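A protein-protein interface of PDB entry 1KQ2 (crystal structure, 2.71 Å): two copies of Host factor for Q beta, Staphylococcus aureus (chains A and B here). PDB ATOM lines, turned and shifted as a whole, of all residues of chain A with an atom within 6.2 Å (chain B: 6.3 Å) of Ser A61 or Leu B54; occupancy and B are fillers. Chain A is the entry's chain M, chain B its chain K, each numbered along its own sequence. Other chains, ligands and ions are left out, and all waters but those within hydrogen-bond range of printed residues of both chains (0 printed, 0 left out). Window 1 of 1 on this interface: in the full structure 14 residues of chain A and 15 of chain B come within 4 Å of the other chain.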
ATOM      1  N   ILE A   7      -7.358  -1.672 -21.428  1.00  0.00           N
ATOM      2  CA  ILE A   7      -6.816  -1.797 -22.773  1.00  0.00           C
ATOM      3  C   ILE A   7      -7.633  -2.861 -23.509  1.00  0.00           C
ATOM      4  O   ILE A   7      -7.997  -2.683 -24.669  1.00  0.00           O
ATOM      5  CB  ILE A   7      -5.326  -2.233 -22.739  1.00  0.00           C
ATOM      6  CG1 ILE A   7      -4.496  -1.209 -21.967  1.00  0.00           C
ATOM      7  CG2 ILE A   7      -4.768  -2.344 -24.152  1.00  0.00           C
ATOM      8  CD1 ILE A   7      -4.378   0.122 -22.663  1.00  0.00           C
ATOM      9  N   GLN A   8      -7.945  -3.955 -22.822  1.00  0.00           N
ATOM     10  CA  GLN A   8      -8.699  -5.040 -23.435  1.00  0.00           C
ATOM     11  C   GLN A   8     -10.082  -4.625 -23.893  1.00  0.00           C
ATOM     12  O   GLN A   8     -10.367  -4.616 -25.081  1.00  0.00           O
ATOM     13  CB  GLN A   8      -8.823  -6.222 -22.473  1.00  0.00           C
ATOM     14  CG  GLN A   8      -9.622  -7.405 -23.037  1.00  0.00           C
ATOM     15  CD  GLN A   8      -9.728  -8.567 -22.056  1.00  0.00           C
ATOM     16  OE1 GLN A   8     -10.385  -9.569 -22.333  1.00  0.00           O
ATOM     17  NE2 GLN A   8      -9.075  -8.438 -20.900  1.00  0.00           N
ATOM     18  N   ALA A  11     -10.514  -2.359 -26.668  1.00  0.00           N
ATOM     19  CA  ALA A  11     -10.066  -2.995 -27.906  1.00  0.00           C
ATOM     20  C   ALA A  11     -11.170  -3.936 -28.394  1.00  0.00           C
ATOM     21  O   ALA A  11     -11.468  -4.010 -29.581  1.00  0.00           O
ATOM     22  CB  ALA A  11      -8.770  -3.770 -27.659  1.00  0.00           C
ATOM     23  N   LEU A  12     -11.776  -4.648 -27.453  1.00  0.00           N
ATOM     24  CA  LEU A  12     -12.852  -5.575 -27.744  1.00  0.00           C
ATOM     25  C   LEU A  12     -14.097  -4.850 -28.235  1.00  0.00           C
ATOM     26  O   LEU A  12     -14.868  -5.390 -29.020  1.00  0.00           O
ATOM     27  CB  LEU A  12     -13.174  -6.389 -26.489  1.00  0.00           C
ATOM     28  CG  LEU A  12     -12.659  -7.831 -26.446  1.00  0.00           C
ATOM     29  CD1 LEU A  12     -11.299  -7.932 -27.127  1.00  0.00           C
ATOM     30  CD2 LEU A  12     -12.597  -8.283 -24.987  1.00  0.00           C
ATOM     31  N   PHE A  15     -13.386  -3.692 -32.065  1.00  0.00           N
ATOM     32  CA  PHE A  15     -13.652  -4.735 -33.056  1.00  0.00           C
ATOM     33  C   PHE A  15     -15.151  -4.958 -33.171  1.00  0.00           C
ATOM     34  O   PHE A  15     -15.693  -5.074 -34.274  1.00  0.00           O
ATOM     35  CB  PHE A  15     -12.992  -6.068 -32.671  1.00  0.00           C
ATOM     36  CG  PHE A  15     -11.510  -5.984 -32.445  1.00  0.00           C
ATOM     37  CD1 PHE A  15     -10.683  -5.342 -33.360  1.00  0.00           C
ATOM     38  CD2 PHE A  15     -10.937  -6.579 -31.321  1.00  0.00           C
ATOM     39  CE1 PHE A  15      -9.304  -5.293 -33.159  1.00  0.00           C
ATOM     40  CE2 PHE A  15      -9.558  -6.537 -31.113  1.00  0.00           C
ATOM     41  CZ  PHE A  15      -8.739  -5.894 -32.032  1.00  0.00           C
ATOM     42  N   VAL A  24      -8.044 -14.851 -34.308  1.00  0.00           N
ATOM     43  CA  VAL A  24      -7.873 -15.251 -32.925  1.00  0.00           C
ATOM     44  C   VAL A  24      -6.921 -16.446 -32.893  1.00  0.00           C
ATOM     45  O   VAL A  24      -7.144 -17.424 -33.595  1.00  0.00           O
ATOM     46  CB  VAL A  24      -9.222 -15.671 -32.302  1.00  0.00           C
ATOM     47  CG1 VAL A  24      -9.083 -15.827 -30.816  1.00  0.00           C
ATOM     48  CG2 VAL A  24     -10.281 -14.647 -32.625  1.00  0.00           C
ATOM     49  N   PHE A  25      -5.857 -16.356 -32.096  1.00  0.00           N
ATOM     50  CA  PHE A  25      -4.892 -17.456 -31.951  1.00  0.00           C
ATOM     51  C   PHE A  25      -5.101 -18.136 -30.599  1.00  0.00           C
ATOM     52  O   PHE A  25      -5.075 -17.478 -29.558  1.00  0.00           O
ATOM     53  CB  PHE A  25      -3.457 -16.939 -32.013  1.00  0.00           C
ATOM     54  CG  PHE A  25      -3.064 -16.401 -33.348  1.00  0.00           C
ATOM     55  CD1 PHE A  25      -2.389 -17.202 -34.263  1.00  0.00           C
ATOM     56  CD2 PHE A  25      -3.354 -15.076 -33.692  1.00  0.00           C
ATOM     57  CE1 PHE A  25      -2.004 -16.698 -35.499  1.00  0.00           C
ATOM     58  CE2 PHE A  25      -2.974 -14.561 -34.924  1.00  0.00           C
ATOM     59  CZ  PHE A  25      -2.295 -15.373 -35.832  1.00  0.00           C
ATOM     60  N   PHE A  26      -5.303 -19.450 -30.616  1.00  0.00           N
ATOM     61  CA  PHE A  26      -5.501 -20.212 -29.390  1.00  0.00           C
ATOM     62  C   PHE A  26      -4.170 -20.667 -28.780  1.00  0.00           C
ATOM     63  O   PHE A  26      -3.127 -20.585 -29.431  1.00  0.00           O
ATOM     64  CB  PHE A  26      -6.378 -21.418 -29.697  1.00  0.00           C
ATOM     65  CG  PHE A  26      -7.755 -21.054 -30.107  1.00  0.00           C
ATOM     66  CD1 PHE A  26      -8.816 -21.202 -29.225  1.00  0.00           C
ATOM     67  CD2 PHE A  26      -7.992 -20.510 -31.362  1.00  0.00           C
ATOM     68  CE1 PHE A  26     -10.106 -20.806 -29.588  1.00  0.00           C
ATOM     69  CE2 PHE A  26      -9.268 -20.109 -31.739  1.00  0.00           C
ATOM     70  CZ  PHE A  26     -10.331 -20.256 -30.845  1.00  0.00           C
ATOM     71  N   LEU A  27      -4.202 -21.148 -27.538  1.00  0.00           N
ATOM     72  CA  LEU A  27      -2.973 -21.619 -26.881  1.00  0.00           C
ATOM     73  C   LEU A  27      -2.433 -22.899 -27.509  1.00  0.00           C
ATOM     74  O   LEU A  27      -1.305 -23.291 -27.259  1.00  0.00           O
ATOM     75  CB  LEU A  27      -3.204 -21.851 -25.393  1.00  0.00           C
ATOM     76  CG  LEU A  27      -3.377 -20.594 -24.544  1.00  0.00           C
ATOM     77  CD1 LEU A  27      -3.845 -20.971 -23.148  1.00  0.00           C
ATOM     78  CD2 LEU A  27      -2.051 -19.857 -24.475  1.00  0.00           C
ATOM     79  N   LYS A  57     -11.857 -17.171 -23.008  1.00  0.00           N
ATOM     80  CA  LYS A  57     -10.629 -16.390 -23.005  1.00  0.00           C
ATOM     81  C   LYS A  57      -9.408 -17.185 -22.543  1.00  0.00           C
ATOM     82  O   LYS A  57      -8.319 -16.987 -23.064  1.00  0.00           O
ATOM     83  CB  LYS A  57     -10.790 -15.142 -22.135  1.00  0.00           C
ATOM     84  CG  LYS A  57     -11.693 -14.112 -22.760  1.00  0.00           C
ATOM     85  CD  LYS A  57     -11.897 -12.953 -21.826  1.00  0.00           C
ATOM     86  CE  LYS A  57     -12.695 -11.838 -22.472  1.00  0.00           C
ATOM     87  NZ  LYS A  57     -12.838 -10.745 -21.484  1.00  0.00           N
ATOM     88  N   ALA A  59      -8.479 -19.845 -23.339  1.00  0.00           N
ATOM     89  CA  ALA A  59      -7.987 -20.622 -24.482  1.00  0.00           C
ATOM     90  C   ALA A  59      -7.408 -19.747 -25.607  1.00  0.00           C
ATOM     91  O   ALA A  59      -6.944 -20.255 -26.630  1.00  0.00           O
ATOM     92  CB  ALA A  59      -9.116 -21.491 -25.031  1.00  0.00           C
ATOM     93  N   ILE A  60      -7.445 -18.434 -25.415  1.00  0.00           N
ATOM     94  CA  ILE A  60      -6.936 -17.499 -26.400  1.00  0.00           C
ATOM     95  C   ILE A  60      -5.605 -16.934 -25.931  1.00  0.00           C
ATOM     96  O   ILE A  60      -5.371 -16.791 -24.728  1.00  0.00           O
ATOM     97  CB  ILE A  60      -7.919 -16.319 -26.605  1.00  0.00           C
ATOM     98  CG1 ILE A  60      -9.216 -16.815 -27.243  1.00  0.00           C
ATOM     99  CG2 ILE A  60      -7.276 -15.233 -27.468  1.00  0.00           C
ATOM    100  CD1 ILE A  60     -10.231 -15.718 -27.436  1.00  0.00           C
ATOM    101  N   SER A  61      -4.727 -16.616 -26.876  1.00  0.00           N
ATOM    102  CA  SER A  61      -3.445 -16.031 -26.523  1.00  0.00           C
ATOM    103  C   SER A  61      -3.240 -14.644 -27.141  1.00  0.00           C
ATOM    104  O   SER A  61      -2.656 -13.771 -26.512  1.00  0.00           O
ATOM    105  CB  SER A  61      -2.294 -16.960 -26.926  1.00  0.00           C
ATOM    106  OG  SER A  61      -2.266 -17.173 -28.316  1.00  0.00           O
ATOM    107  N   THR A  62      -3.740 -14.436 -28.354  1.00  0.00           N
ATOM    108  CA  THR A  62      -3.568 -13.162 -29.038  1.00  0.00           C
ATOM    109  C   THR A  62      -4.694 -12.823 -30.019  1.00  0.00           C
ATOM    110  O   THR A  62      -5.370 -13.713 -30.533  1.00  0.00           O
ATOM    111  CB  THR A  62      -2.252 -13.152 -29.853  1.00  0.00           C
ATOM    112  OG1 THR A  62      -1.175 -13.611 -29.038  1.00  0.00           O
ATOM    113  CG2 THR A  62      -1.921 -11.750 -30.317  1.00  0.00           C
ATOM    114  N   TYR A  63      -4.878 -11.526 -30.262  1.00  0.00           N
ATOM    115  CA  TYR A  63      -5.842 -11.006 -31.228  1.00  0.00           C
ATOM    116  C   TYR A  63      -4.995 -10.125 -32.155  1.00  0.00           C
ATOM    117  O   TYR A  63      -4.066  -9.454 -31.688  1.00  0.00           O
ATOM    118  CB  TYR A  63      -6.877 -10.083 -30.587  1.00  0.00           C
ATOM    119  CG  TYR A  63      -7.784 -10.672 -29.534  1.00  0.00           C
ATOM    120  CD1 TYR A  63      -8.987 -11.291 -29.879  1.00  0.00           C
ATOM    121  CD2 TYR A  63      -7.484 -10.523 -28.186  1.00  0.00           C
ATOM    122  CE1 TYR A  63      -9.873 -11.734 -28.904  1.00  0.00           C
ATOM    123  CE2 TYR A  63      -8.361 -10.960 -27.209  1.00  0.00           C
ATOM    124  CZ  TYR A  63      -9.553 -11.556 -27.568  1.00  0.00           C
ATOM    125  OH  TYR A  63     -10.436 -11.907 -26.575  1.00  0.00           O
ATOM    126  N   THR A  64      -5.308 -10.141 -33.451  1.00  0.00           N
ATOM    127  CA  THR A  64      -4.631  -9.326 -34.462  1.00  0.00           C
ATOM    128  C   THR A  64      -5.549  -9.236 -35.685  1.00  0.00           C
ATOM    129  O   THR A  64      -6.528  -9.980 -35.795  1.00  0.00           O
ATOM    130  CB  THR A  64      -3.276  -9.930 -34.940  1.00  0.00           C
ATOM    131  OG1 THR A  64      -3.518 -10.913 -35.948  1.00  0.00           O
ATOM    132  CG2 THR A  64      -2.537 -10.594 -33.797  1.00  0.00           C
ATOM    133  N   PHE B  26       5.857 -17.480 -25.352  1.00  0.00           N
ATOM    134  CA  PHE B  26       4.561 -17.984 -24.906  1.00  0.00           C
ATOM    135  C   PHE B  26       4.715 -19.385 -24.315  1.00  0.00           C
ATOM    136  O   PHE B  26       5.759 -20.024 -24.464  1.00  0.00           O
ATOM    137  CB  PHE B  26       3.570 -18.050 -26.069  1.00  0.00           C
ATOM    138  CG  PHE B  26       3.257 -16.728 -26.683  1.00  0.00           C
ATOM    139  CD1 PHE B  26       1.939 -16.319 -26.823  1.00  0.00           C
ATOM    140  CD2 PHE B  26       4.272 -15.891 -27.136  1.00  0.00           C
ATOM    141  CE1 PHE B  26       1.629 -15.087 -27.412  1.00  0.00           C
ATOM    142  CE2 PHE B  26       3.974 -14.653 -27.727  1.00  0.00           C
ATOM    143  CZ  PHE B  26       2.651 -14.255 -27.863  1.00  0.00           C
ATOM    144  N   ASN B  28       3.070 -22.092 -25.228  1.00  0.00           N
ATOM    145  CA  ASN B  28       3.056 -23.101 -26.292  1.00  0.00           C
ATOM    146  C   ASN B  28       4.313 -23.138 -27.165  1.00  0.00           C
ATOM    147  O   ASN B  28       4.350 -23.890 -28.143  1.00  0.00           O
ATOM    148  CB  ASN B  28       1.831 -22.913 -27.214  1.00  0.00           C
ATOM    149  CG  ASN B  28       1.720 -21.499 -27.775  1.00  0.00           C
ATOM    150  OD1 ASN B  28       2.713 -20.762 -27.873  1.00  0.00           O
ATOM    151  ND2 ASN B  28       0.507 -21.118 -28.162  1.00  0.00           N
ATOM    152  N   PHE B  30       5.505 -20.508 -28.856  1.00  0.00           N
ATOM    153  CA  PHE B  30       5.470 -19.460 -29.851  1.00  0.00           C
ATOM    154  C   PHE B  30       6.181 -18.208 -29.308  1.00  0.00           C
ATOM    155  O   PHE B  30       6.413 -18.072 -28.103  1.00  0.00           O
ATOM    156  CB  PHE B  30       4.018 -19.121 -30.182  1.00  0.00           C
ATOM    157  CG  PHE B  30       3.873 -18.104 -31.264  1.00  0.00           C
ATOM    158  CD1 PHE B  30       4.376 -18.352 -32.543  1.00  0.00           C
ATOM    159  CD2 PHE B  30       3.234 -16.894 -31.017  1.00  0.00           C
ATOM    160  CE1 PHE B  30       4.247 -17.406 -33.566  1.00  0.00           C
ATOM    161  CE2 PHE B  30       3.097 -15.933 -32.041  1.00  0.00           C
ATOM    162  CZ  PHE B  30       3.605 -16.195 -33.318  1.00  0.00           C
ATOM    163  N   VAL B  43      -4.177  -7.935 -20.224  1.00  0.00           N
ATOM    164  CA  VAL B  43      -3.506  -7.986 -21.508  1.00  0.00           C
ATOM    165  C   VAL B  43      -2.232  -7.161 -21.578  1.00  0.00           C
ATOM    166  O   VAL B  43      -1.799  -6.559 -20.604  1.00  0.00           O
ATOM    167  CB  VAL B  43      -4.442  -7.519 -22.651  1.00  0.00           C
ATOM    168  CG1 VAL B  43      -5.686  -8.383 -22.685  1.00  0.00           C
ATOM    169  CG2 VAL B  43      -4.806  -6.047 -22.476  1.00  0.00           C
ATOM    170  N   VAL B  44      -1.633  -7.170 -22.760  1.00  0.00           N
ATOM    171  CA  VAL B  44      -0.420  -6.427 -23.063  1.00  0.00           C
ATOM    172  C   VAL B  44      -0.502  -6.186 -24.563  1.00  0.00           C
ATOM    173  O   VAL B  44      -0.714  -7.120 -25.330  1.00  0.00           O
ATOM    174  CB  VAL B  44       0.857  -7.240 -22.760  1.00  0.00           C
ATOM    175  CG1 VAL B  44       1.999  -6.677 -23.539  1.00  0.00           C
ATOM    176  CG2 VAL B  44       1.188  -7.186 -21.277  1.00  0.00           C
ATOM    177  N   SER B  45      -0.381  -4.930 -24.974  1.00  0.00           N
ATOM    178  CA  SER B  45      -0.431  -4.606 -26.389  1.00  0.00           C
ATOM    179  C   SER B  45       0.994  -4.565 -26.904  1.00  0.00           C
ATOM    180  O   SER B  45       1.831  -3.837 -26.371  1.00  0.00           O
ATOM    181  CB  SER B  45      -1.091  -3.265 -26.607  1.00  0.00           C
ATOM    182  OG  SER B  45      -1.120  -2.987 -27.990  1.00  0.00           O
ATOM    183  N   LEU B  46       1.278  -5.357 -27.931  1.00  0.00           N
ATOM    184  CA  LEU B  46       2.630  -5.421 -28.468  1.00  0.00           C
ATOM    185  C   LEU B  46       2.703  -5.048 -29.928  1.00  0.00           C
ATOM    186  O   LEU B  46       2.040  -5.651 -30.764  1.00  0.00           O
ATOM    187  CB  LEU B  46       3.202  -6.829 -28.286  1.00  0.00           C
ATOM    188  CG  LEU B  46       4.669  -6.988 -28.696  1.00  0.00           C
ATOM    189  CD1 LEU B  46       5.525  -7.065 -27.445  1.00  0.00           C
ATOM    190  CD2 LEU B  46       4.866  -8.232 -29.533  1.00  0.00           C
ATOM    191  N   GLN B  52      -0.320  -4.482 -34.770  1.00  0.00           N
ATOM    192  CA  GLN B  52      -0.674  -4.474 -33.359  1.00  0.00           C
ATOM    193  C   GLN B  52      -1.204  -5.836 -32.920  1.00  0.00           C
ATOM    194  O   GLN B  52      -2.139  -6.373 -33.516  1.00  0.00           O
ATOM    195  CB  GLN B  52      -1.732  -3.404 -33.104  1.00  0.00           C
ATOM    196  CG  GLN B  52      -1.698  -2.800 -31.715  1.00  0.00           C
ATOM    197  CD  GLN B  52      -0.403  -2.055 -31.444  1.00  0.00           C
ATOM    198  OE1 GLN B  52       0.055  -1.258 -32.268  1.00  0.00           O
ATOM    199  NE2 GLN B  52       0.192  -2.305 -30.280  1.00  0.00           N
ATOM    200  N   HIS B  53      -0.601  -6.381 -31.866  1.00  0.00           N
ATOM    201  CA  HIS B  53      -0.995  -7.677 -31.324  1.00  0.00           C
ATOM    202  C   HIS B  53      -1.460  -7.530 -29.873  1.00  0.00           C
ATOM    203  O   HIS B  53      -0.717  -7.021 -29.037  1.00  0.00           O
ATOM    204  CB  HIS B  53       0.196  -8.641 -31.389  1.00  0.00           C
ATOM    205  CG  HIS B  53       0.731  -8.849 -32.773  1.00  0.00           C
ATOM    206  ND1 HIS B  53       0.078  -9.611 -33.718  1.00  0.00           N
ATOM    207  CD2 HIS B  53       1.836  -8.360 -33.385  1.00  0.00           C
ATOM    208  CE1 HIS B  53       0.757  -9.582 -34.853  1.00  0.00           C
ATOM    209  NE2 HIS B  53       1.826  -8.829 -34.677  1.00  0.00           N
ATOM    210  N   LEU B  54      -2.682  -7.964 -29.572  1.00  0.00           N
ATOM    211  CA  LEU B  54      -3.192  -7.886 -28.200  1.00  0.00           C
ATOM    212  C   LEU B  54      -2.939  -9.253 -27.547  1.00  0.00           C
ATOM    213  O   LEU B  54      -3.465 -10.271 -27.991  1.00  0.00           O
ATOM    214  CB  LEU B  54      -4.688  -7.537 -28.216  1.00  0.00           C
ATOM    215  CG  LEU B  54      -5.370  -7.104 -26.905  1.00  0.00           C
ATOM    216  CD1 LEU B  54      -4.592  -5.996 -26.212  1.00  0.00           C
ATOM    217  CD2 LEU B  54      -6.777  -6.625 -27.223  1.00  0.00           C
ATOM    218  N   ILE B  55      -2.135  -9.278 -26.488  1.00  0.00           N
ATOM    219  CA  ILE B  55      -1.761 -10.540 -25.848  1.00  0.00           C
ATOM    220  C   ILE B  55      -2.234 -10.764 -24.420  1.00  0.00           C
ATOM    221  O   ILE B  55      -1.986  -9.937 -23.560  1.00  0.00           O
ATOM    222  CB  ILE B  55      -0.200 -10.699 -25.815  1.00  0.00           C
ATOM    223  CG1 ILE B  55       0.403 -10.457 -27.206  1.00  0.00           C
ATOM    224  CG2 ILE B  55       0.176 -12.090 -25.310  1.00  0.00           C
ATOM    225  CD1 ILE B  55       1.938 -10.351 -27.218  1.00  0.00           C
ATOM    226  N   TYR B  56      -2.889 -11.892 -24.162  1.00  0.00           N
ATOM    227  CA  TYR B  56      -3.309 -12.231 -22.802  1.00  0.00           C
ATOM    228  C   TYR B  56      -2.071 -12.654 -22.004  1.00  0.00           C
ATOM    229  O   TYR B  56      -1.249 -13.431 -22.483  1.00  0.00           O
ATOM    230  CB  TYR B  56      -4.301 -13.390 -22.810  1.00  0.00           C
ATOM    231  CG  TYR B  56      -5.704 -12.984 -23.150  1.00  0.00           C
ATOM    232  CD1 TYR B  56      -6.463 -12.229 -22.260  1.00  0.00           C
ATOM    233  CD2 TYR B  56      -6.252 -13.301 -24.383  1.00  0.00           C
ATOM    234  CE1 TYR B  56      -7.730 -11.793 -22.601  1.00  0.00           C
ATOM    235  CE2 TYR B  56      -7.517 -12.876 -24.734  1.00  0.00           C
ATOM    236  CZ  TYR B  56      -8.256 -12.116 -23.844  1.00  0.00           C
ATOM    237  OH  TYR B  56      -9.502 -11.652 -24.224  1.00  0.00           O
ATOM    238  N   LYS B  57      -1.930 -12.146 -20.789  1.00  0.00           N
ATOM    239  CA  LYS B  57      -0.783 -12.497 -19.972  1.00  0.00           C
ATOM    240  C   LYS B  57      -0.824 -13.966 -19.585  1.00  0.00           C
ATOM    241  O   LYS B  57       0.215 -14.563 -19.317  1.00  0.00           O
ATOM    242  CB  LYS B  57      -0.746 -11.657 -18.692  1.00  0.00           C
ATOM    243  CG  LYS B  57      -0.499 -10.180 -18.883  1.00  0.00           C
ATOM    244  CD  LYS B  57      -0.508  -9.497 -17.536  1.00  0.00           C
ATOM    245  CE  LYS B  57      -0.222  -8.020 -17.663  1.00  0.00           C
ATOM    246  NZ  LYS B  57      -0.243  -7.350 -16.341  1.00  0.00           N
ATOM    247  N   HIS B  58      -2.016 -14.557 -19.541  1.00  0.00           N
ATOM    248  CA  HIS B  58      -2.102 -15.962 -19.164  1.00  0.00           C
ATOM    249  C   HIS B  58      -1.436 -16.892 -20.184  1.00  0.00           C
ATOM    250  O   HIS B  58      -1.248 -18.081 -19.926  1.00  0.00           O
ATOM    251  CB  HIS B  58      -3.567 -16.377 -18.892  1.00  0.00           C
ATOM    252  CG  HIS B  58      -4.467 -16.343 -20.090  1.00  0.00           C
ATOM    253  ND1 HIS B  58      -5.717 -15.760 -20.057  1.00  0.00           N
ATOM    254  CD2 HIS B  58      -4.329 -16.864 -21.334  1.00  0.00           C
ATOM    255  CE1 HIS B  58      -6.307 -15.922 -21.229  1.00  0.00           C
ATOM    256  NE2 HIS B  58      -5.487 -16.588 -22.022  1.00  0.00           N
ATOM    257  N   ALA B  59      -1.050 -16.327 -21.322  1.00  0.00           N
ATOM    258  CA  ALA B  59      -0.418 -17.069 -22.399  1.00  0.00           C
ATOM    259  C   ALA B  59       1.078 -16.811 -22.453  1.00  0.00           C
ATOM    260  O   ALA B  59       1.850 -17.638 -22.945  1.00  0.00           O
ATOM    261  CB  ALA B  59      -1.057 -16.683 -23.717  1.00  0.00           C
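Positions printed for both chains: 26, 57 and 59.
Of the 24 pairs that touch across the chains among the printed residues, none has its exchanged pair printed and touching as well.
Of the 16 printed residues of chain A, 11 touch a printed residue of chain B.
Among the printed residues, 24 pairs touch across the chains.
Of chain B, only Leu B54, Ile B55, Tyr B56 and Ala B59 come within 4 Å of Ser A61.
Of the printed residues of chain A, Leu B54 touches Ala A11, Ser A61, Thr A62 and Tyr A63.
Of the printed residues of chain B, Leu A27 touches Asn B28 and Ala B59.
Printed residues of chain A within 4 Å of Gln B52: Thr A64 (3.98 Å).
Of the printed residues of chain A, Val B43 touches Ile A7 (3.9 Å) and Gln A8 (3.8 Å).
Of the printed residues of chain B, Ile A7 touches Val B43.
Of the printed residues of chain B, Lys A57 touches Tyr B56 and His B58.
Ser B45 touches none of the printed residues of chain A.
The nearest residue of chain B that does not touch Ser A61 is Phe B26 (4.3 Å).
The nearest residue of chain A that does not touch Leu B54 is Ile A7 (4.2 Å).
The nearest printed residue of chain B that does not touch Phe A26 is Phe B26 (7.1 Å).
CB of Ile A7 touches CG2 of Val B43, at 3.9 Å.
CB of Ala A11 touches CD2 of Leu B54, 3.5 Å away.
Leu A27 touches Ala B59 (CD2 to CB, 3.4 Å).
CD2 of Tyr B56 touches O of Ile A60 (3.6 Å).
O of Ser A61 touches O of Leu B54, 3.9 Å away.
CA of Ile B55 touches O of Ser A61, at 3.4 Å.
Phe B26 touches Thr A62.
CG2 of Thr A62 touches CB of His B53, 3.9 Å away.
Leu B54 touches Thr A62.
Gln B52 touches Thr A64 (O to CA, 3.98 Å).
The backbone NH (N) of Tyr B56 is in hydrogen-bond range of the backbone carbonyl oxygen (O) of Ser A61, 3.0 Å away.
A ring nitrogen (NE2) of His B58 sits close to the backbone carbonyl oxygen (O) of Lys A57 (3.0 Å).
The backbone carbonyl oxygen of Ile A60 is in hydrogen-bond range of a ring nitrogen (NE2) of His B58, at 2.7 Å.
The side-chain amide nitrogen (ND2) of Asn B28 lies within hydrogen-bond range of the backbone carbonyl oxygen (O) of Leu A27.
The backbone NH (N) of Leu B54 is in hydrogen-bond range of the backbone carbonyl oxygen (O) of Tyr A63 (2.9 Å).
The side-chain hydroxyl of Tyr B56 lies within hydrogen-bond range of the side-chain hydroxyl of Tyr A63 (2.5 Å).
The side-chain hydroxyl (OH) of Tyr B56 is in hydrogen-bond range of the side-chain amide oxygen (OE1) of Gln A8 (2.9 Å).
O of Val B44 is in hydrogen-bond range of N of Ile B55.
The side-chain amide oxygen (OE1) of Gln A8 is in hydrogen-bond range of the side-chain amino group (NZ) of Lys A57, 2.8 Å away.
The side-chain amide oxygen of Asn B28 lies within hydrogen-bond range of the backbone NH of Phe B30, 3.0 Å away.
The backbone carbonyl oxygen of Thr A62 is in hydrogen-bond range of the backbone NH of Phe A25.
The backbone carbonyl oxygen of Phe A25 is in hydrogen-bond range of the backbone NH of Ser A61 (2.8 Å).
The backbone carbonyl oxygen of Ala A59 sits at hydrogen-bond distance from the backbone NH of Leu A27, at 3.0 Å.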
